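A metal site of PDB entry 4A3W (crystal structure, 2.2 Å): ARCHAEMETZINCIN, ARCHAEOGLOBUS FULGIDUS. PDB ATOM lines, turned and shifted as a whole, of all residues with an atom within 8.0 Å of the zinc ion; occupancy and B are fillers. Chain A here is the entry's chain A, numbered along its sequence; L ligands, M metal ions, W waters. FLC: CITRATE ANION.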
ATOM      1  N   GLY A  83     -11.071  18.018  -0.696  1.00  0.00           N
ATOM      2  CA  GLY A  83     -11.388  17.067  -1.738  1.00  0.00           C
ATOM      3  C   GLY A  83     -12.573  17.525  -2.574  1.00  0.00           C
ATOM      4  O   GLY A  83     -13.011  18.659  -2.470  1.00  0.00           O
ATOM      5  N   GLU A  84     -13.077  16.629  -3.411  1.00  0.00           N
ATOM      6  CA  GLU A  84     -14.194  16.930  -4.285  1.00  0.00           C
ATOM      7  C   GLU A  84     -14.790  15.641  -4.828  1.00  0.00           C
ATOM      8  O   GLU A  84     -14.057  14.735  -5.229  1.00  0.00           O
ATOM      9  CB  GLU A  84     -13.754  17.825  -5.451  1.00  0.00           C
ATOM     10  CG  GLU A  84     -14.922  18.160  -6.401  1.00  0.00           C
ATOM     11  CD  GLU A  84     -14.573  19.174  -7.479  1.00  0.00           C
ATOM     12  OE1 GLU A  84     -13.490  19.785  -7.404  1.00  0.00           O
ATOM     13  OE2 GLU A  84     -15.375  19.361  -8.412  1.00  0.00           O
ATOM     14  N   ALA A  85     -16.111  15.555  -4.862  1.00  0.00           N
ATOM     15  CA  ALA A  85     -16.788  14.356  -5.322  1.00  0.00           C
ATOM     16  C   ALA A  85     -17.895  14.684  -6.308  1.00  0.00           C
ATOM     17  O   ALA A  85     -18.495  15.763  -6.257  1.00  0.00           O
ATOM     18  CB  ALA A  85     -17.371  13.594  -4.131  1.00  0.00           C
ATOM     19  N   GLU A 114     -12.438  11.726   5.957  1.00  0.00           N
ATOM     20  CA  GLU A 114     -12.634  12.540   4.767  1.00  0.00           C
ATOM     21  C   GLU A 114     -12.827  11.653   3.533  1.00  0.00           C
ATOM     22  O   GLU A 114     -13.567  12.015   2.629  1.00  0.00           O
ATOM     23  CB  GLU A 114     -11.474  13.526   4.567  1.00  0.00           C
ATOM     24  CG  GLU A 114     -11.449  14.676   5.594  1.00  0.00           C
ATOM     25  CD  GLU A 114     -12.736  15.491   5.571  1.00  0.00           C
ATOM     26  OE1 GLU A 114     -12.843  16.443   4.767  1.00  0.00           O
ATOM     27  OE2 GLU A 114     -13.661  15.176   6.341  1.00  0.00           O
ATOM     28  N   HIS A 117     -16.389  10.551   3.822  1.00  0.00           N
ATOM     29  CA  HIS A 117     -17.207  11.699   3.454  1.00  0.00           C
ATOM     30  C   HIS A 117     -17.341  11.805   1.923  1.00  0.00           C
ATOM     31  O   HIS A 117     -18.436  11.912   1.400  1.00  0.00           O
ATOM     32  CB  HIS A 117     -16.582  12.974   4.049  1.00  0.00           C
ATOM     33  CG  HIS A 117     -17.306  14.237   3.691  1.00  0.00           C
ATOM     34  ND1 HIS A 117     -18.158  14.889   4.565  1.00  0.00           N
ATOM     35  CD2 HIS A 117     -17.273  14.995   2.563  1.00  0.00           C
ATOM     36  CE1 HIS A 117     -18.627  15.983   3.988  1.00  0.00           C
ATOM     37  NE2 HIS A 117     -18.119  16.067   2.772  1.00  0.00           N
ATOM     38  N   GLU A 118     -16.208  11.773   1.220  1.00  0.00           N
ATOM     39  CA  GLU A 118     -16.205  11.931  -0.230  1.00  0.00           C
ATOM     40  C   GLU A 118     -16.977  10.789  -0.902  1.00  0.00           C
ATOM     41  O   GLU A 118     -17.741  11.016  -1.836  1.00  0.00           O
ATOM     42  CB  GLU A 118     -14.780  12.007  -0.783  1.00  0.00           C
ATOM     43  CG  GLU A 118     -13.963  13.217  -0.326  1.00  0.00           C
ATOM     44  CD  GLU A 118     -14.524  14.564  -0.828  1.00  0.00           C
ATOM     45  OE1 GLU A 118     -15.419  14.579  -1.691  1.00  0.00           O
ATOM     46  OE2 GLU A 118     -14.064  15.619  -0.329  1.00  0.00           O
ATOM     47  N   GLY A 120     -19.336   8.975   0.497  1.00  0.00           N
ATOM     48  CA  GLY A 120     -20.729   9.229   0.804  1.00  0.00           C
ATOM     49  C   GLY A 120     -21.385  10.101  -0.252  1.00  0.00           C
ATOM     50  O   GLY A 120     -22.485   9.794  -0.718  1.00  0.00           O
ATOM     51  N   HIS A 121     -20.703  11.175  -0.645  1.00  0.00           N
ATOM     52  CA  HIS A 121     -21.194  12.047  -1.729  1.00  0.00           C
ATOM     53  C   HIS A 121     -21.375  11.262  -3.031  1.00  0.00           C
ATOM     54  O   HIS A 121     -22.377  11.415  -3.726  1.00  0.00           O
ATOM     55  CB  HIS A 121     -20.202  13.175  -2.029  1.00  0.00           C
ATOM     56  CG  HIS A 121     -20.280  14.327  -1.092  1.00  0.00           C
ATOM     57  ND1 HIS A 121     -21.470  14.903  -0.714  1.00  0.00           N
ATOM     58  CD2 HIS A 121     -19.300  15.058  -0.479  1.00  0.00           C
ATOM     59  CE1 HIS A 121     -21.230  15.917   0.104  1.00  0.00           C
ATOM     60  NE2 HIS A 121     -19.922  16.033   0.262  1.00  0.00           N
ATOM     61  N   LEU A 125     -25.155  11.079  -1.039  1.00  0.00           N
ATOM     62  CA  LEU A 125     -25.434  11.852   0.188  1.00  0.00           C
ATOM     63  C   LEU A 125     -24.985  13.295   0.069  1.00  0.00           C
ATOM     64  O   LEU A 125     -23.860  13.594  -0.378  1.00  0.00           O
ATOM     65  CB  LEU A 125     -24.775  11.211   1.413  1.00  0.00           C
ATOM     66  CG  LEU A 125     -25.215   9.799   1.817  1.00  0.00           C
ATOM     67  CD1 LEU A 125     -24.358   9.252   2.968  1.00  0.00           C
ATOM     68  CD2 LEU A 125     -26.692   9.772   2.191  1.00  0.00           C
ATOM     69  N   LYS A 126     -25.852  14.205   0.480  1.00  0.00           N
ATOM     70  CA  LYS A 126     -25.485  15.610   0.563  1.00  0.00           C
ATOM     71  C   LYS A 126     -24.958  15.914   1.968  1.00  0.00           C
ATOM     72  O   LYS A 126     -24.932  15.035   2.830  1.00  0.00           O
ATOM     73  CB  LYS A 126     -26.689  16.509   0.290  1.00  0.00           C
ATOM     74  CG  LYS A 126     -27.261  16.379  -1.114  1.00  0.00           C
ATOM     75  CD  LYS A 126     -28.464  17.305  -1.294  1.00  0.00           C
ATOM     76  CE  LYS A 126     -29.444  16.769  -2.319  1.00  0.00           C
ATOM     77  NZ  LYS A 126     -30.842  17.241  -2.047  1.00  0.00           N
ATOM     78  N   HIS A 127     -24.580  17.150   2.198  1.00  0.00           N
ATOM     79  CA  HIS A 127     -24.151  17.534   3.520  1.00  0.00           C
ATOM     80  C   HIS A 127     -25.267  17.365   4.554  1.00  0.00           C
ATOM     81  O   HIS A 127     -26.460  17.479   4.253  1.00  0.00           O
ATOM     82  CB  HIS A 127     -23.614  18.956   3.512  1.00  0.00           C
ATOM     83  CG  HIS A 127     -22.251  19.047   2.880  1.00  0.00           C
ATOM     84  ND1 HIS A 127     -21.811  20.165   2.212  1.00  0.00           N
ATOM     85  CD2 HIS A 127     -21.254  18.142   2.810  1.00  0.00           C
ATOM     86  CE1 HIS A 127     -20.612  19.944   1.741  1.00  0.00           C
ATOM     87  NE2 HIS A 127     -20.244  18.730   2.089  1.00  0.00           N
ATOM     88  N   CYS A 128     -24.839  17.053   5.772  1.00  0.00           N
ATOM     89  CA  CYS A 128     -25.739  16.693   6.854  1.00  0.00           C
ATOM     90  C   CYS A 128     -25.444  17.617   8.015  1.00  0.00           C
ATOM     91  O   CYS A 128     -24.284  17.956   8.258  1.00  0.00           O
ATOM     92  CB  CYS A 128     -25.467  15.247   7.252  1.00  0.00           C
ATOM     93  SG  CYS A 128     -26.481  14.627   8.583  1.00  0.00           S
ATOM     94  N   VAL A 133     -20.466  11.969   9.789  1.00  0.00           N
ATOM     95  CA  VAL A 133     -19.318  12.125   8.911  1.00  0.00           C
ATOM     96  C   VAL A 133     -19.652  13.019   7.697  1.00  0.00           C
ATOM     97  O   VAL A 133     -18.749  13.631   7.110  1.00  0.00           O
ATOM     98  CB  VAL A 133     -18.787  10.740   8.442  1.00  0.00           C
ATOM     99  CG1 VAL A 133     -19.778  10.071   7.438  1.00  0.00           C
ATOM    100  CG2 VAL A 133     -17.384  10.872   7.843  1.00  0.00           C
ATOM    101  N   MET A 134     -20.934  13.130   7.345  1.00  0.00           N
ATOM    102  CA  MET A 134     -21.324  13.932   6.166  1.00  0.00           C
ATOM    103  C   MET A 134     -21.447  15.451   6.447  1.00  0.00           C
ATOM    104  O   MET A 134     -21.767  16.250   5.552  1.00  0.00           O
ATOM    105  CB  MET A 134     -22.637  13.418   5.551  1.00  0.00           C
ATOM    106  CG  MET A 134     -22.515  12.063   4.836  1.00  0.00           C
ATOM    107  SD  MET A 134     -21.112  11.991   3.692  1.00  0.00           S
ATOM    108  CE  MET A 134     -21.393  13.432   2.658  1.00  0.00           C
ATOM    109  N   ARG A 135     -21.160  15.854   7.667  1.00  0.00           N
ATOM    110  CA  ARG A 135     -21.092  17.263   8.011  1.00  0.00           C
ATOM    111  C   ARG A 135     -19.998  17.930   7.180  1.00  0.00           C
ATOM    112  O   ARG A 135     -18.936  17.352   6.961  1.00  0.00           O
ATOM    113  CB  ARG A 135     -20.787  17.397   9.505  1.00  0.00           C
ATOM    114  CG  ARG A 135     -20.922  18.785  10.052  1.00  0.00           C
ATOM    115  CD  ARG A 135     -20.631  18.821  11.544  1.00  0.00           C
ATOM    116  NE  ARG A 135     -21.765  18.361  12.338  1.00  0.00           N
ATOM    117  CZ  ARG A 135     -21.734  18.214  13.663  1.00  0.00           C
ATOM    118  NH1 ARG A 135     -20.632  18.471  14.350  1.00  0.00           N
ATOM    119  NH2 ARG A 135     -22.824  17.797  14.301  1.00  0.00           N
ATOM    120  N   PHE A 136     -20.267  19.134   6.679  1.00  0.00           N
ATOM    121  CA  PHE A 136     -19.237  19.962   6.071  1.00  0.00           C
ATOM    122  C   PHE A 136     -18.226  20.406   7.124  1.00  0.00           C
ATOM    123  O   PHE A 136     -18.606  20.768   8.233  1.00  0.00           O
ATOM    124  CB  PHE A 136     -19.865  21.200   5.435  1.00  0.00           C
ATOM    125  CG  PHE A 136     -18.851  22.216   4.973  1.00  0.00           C
ATOM    126  CD1 PHE A 136     -18.267  22.099   3.715  1.00  0.00           C
ATOM    127  CD2 PHE A 136     -18.490  23.277   5.788  1.00  0.00           C
ATOM    128  CE1 PHE A 136     -17.319  23.030   3.282  1.00  0.00           C
ATOM    129  CE2 PHE A 136     -17.549  24.209   5.371  1.00  0.00           C
ATOM    130  CZ  PHE A 136     -16.966  24.100   4.125  1.00  0.00           C
ATOM    131  N   SER A 137     -16.942  20.372   6.786  1.00  0.00           N
ATOM    132  CA  SER A 137     -15.883  20.831   7.694  1.00  0.00           C
ATOM    133  C   SER A 137     -15.177  22.035   7.122  1.00  0.00           C
ATOM    134  O   SER A 137     -14.564  21.956   6.044  1.00  0.00           O
ATOM    135  CB  SER A 137     -14.842  19.737   7.940  1.00  0.00           C
ATOM    136  OG  SER A 137     -15.437  18.630   8.595  1.00  0.00           O
ATOM    137  N   LYS A 146     -16.170  16.071  13.907  1.00  0.00           N
ATOM    138  CA  LYS A 146     -17.239  15.190  13.409  1.00  0.00           C
ATOM    139  C   LYS A 146     -16.832  13.726  13.551  1.00  0.00           C
ATOM    140  O   LYS A 146     -15.644  13.409  13.578  1.00  0.00           O
ATOM    141  CB  LYS A 146     -17.648  15.529  11.969  1.00  0.00           C
ATOM    142  CG  LYS A 146     -16.656  15.129  10.879  1.00  0.00           C
ATOM    143  CD  LYS A 146     -17.100  15.709   9.514  1.00  0.00           C
ATOM    144  CE  LYS A 146     -16.112  15.386   8.390  1.00  0.00           C
ATOM    145  NZ  LYS A 146     -16.277  16.303   7.191  1.00  0.00           N
HETATM  146  CAC FLC L   1     -13.975  20.262   1.066  1.00  0.00           C
HETATM  147  CA  FLC L   1     -15.455  20.212   1.301  1.00  0.00           C
HETATM  148  CB  FLC L   1     -16.008  18.843   1.564  1.00  0.00           C
HETATM  149  CBC FLC L   1     -16.045  18.021   0.317  1.00  0.00           C
HETATM  150  CG  FLC L   1     -15.201  18.047   2.539  1.00  0.00           C
HETATM  151  CGC FLC L   1     -15.566  18.327   3.966  1.00  0.00           C
HETATM  152  OA1 FLC L   1     -13.267  21.099   1.677  1.00  0.00           O
HETATM  153  OA2 FLC L   1     -13.414  19.499   0.241  1.00  0.00           O
HETATM  154  OB1 FLC L   1     -15.049  17.938  -0.466  1.00  0.00           O
HETATM  155  OB2 FLC L   1     -17.094  17.383   0.082  1.00  0.00           O
HETATM  156  OG1 FLC L   1     -16.490  19.127   4.262  1.00  0.00           O
HETATM  157  OG2 FLC L   1     -14.899  17.788   4.893  1.00  0.00           O
HETATM  158  OHB FLC L   1     -17.314  19.013   2.006  1.00  0.00           O
HETATM  159 ZN    ZN M   1     -18.766  17.422   1.376  1.00  0.00          ZN
HETATM  160  O   HOH W   1     -18.777  19.467  -0.693  1.00  0.00           O
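Three residues have an atom within 4 Å of the zinc ion: His 117, His 121 and His 127.
A ring nitrogen (NE2) of His 117 binds the zinc ion, at 2.1 Å.
NE2 of His 127 is bound to the zinc ion (2.1 Å).
OB2 of the ligand binds the zinc ion, 2.1 Å away.
NE2 of His 121 is bound to the zinc ion.
The zinc ion is bound by OHB of the ligand, 2.2 Å away.
ND1 of His 121 lies within hydrogen-bond range of O of Leu 125.
ND1 of His 117 is in hydrogen-bond range of O of Val 133 (2.9 Å).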
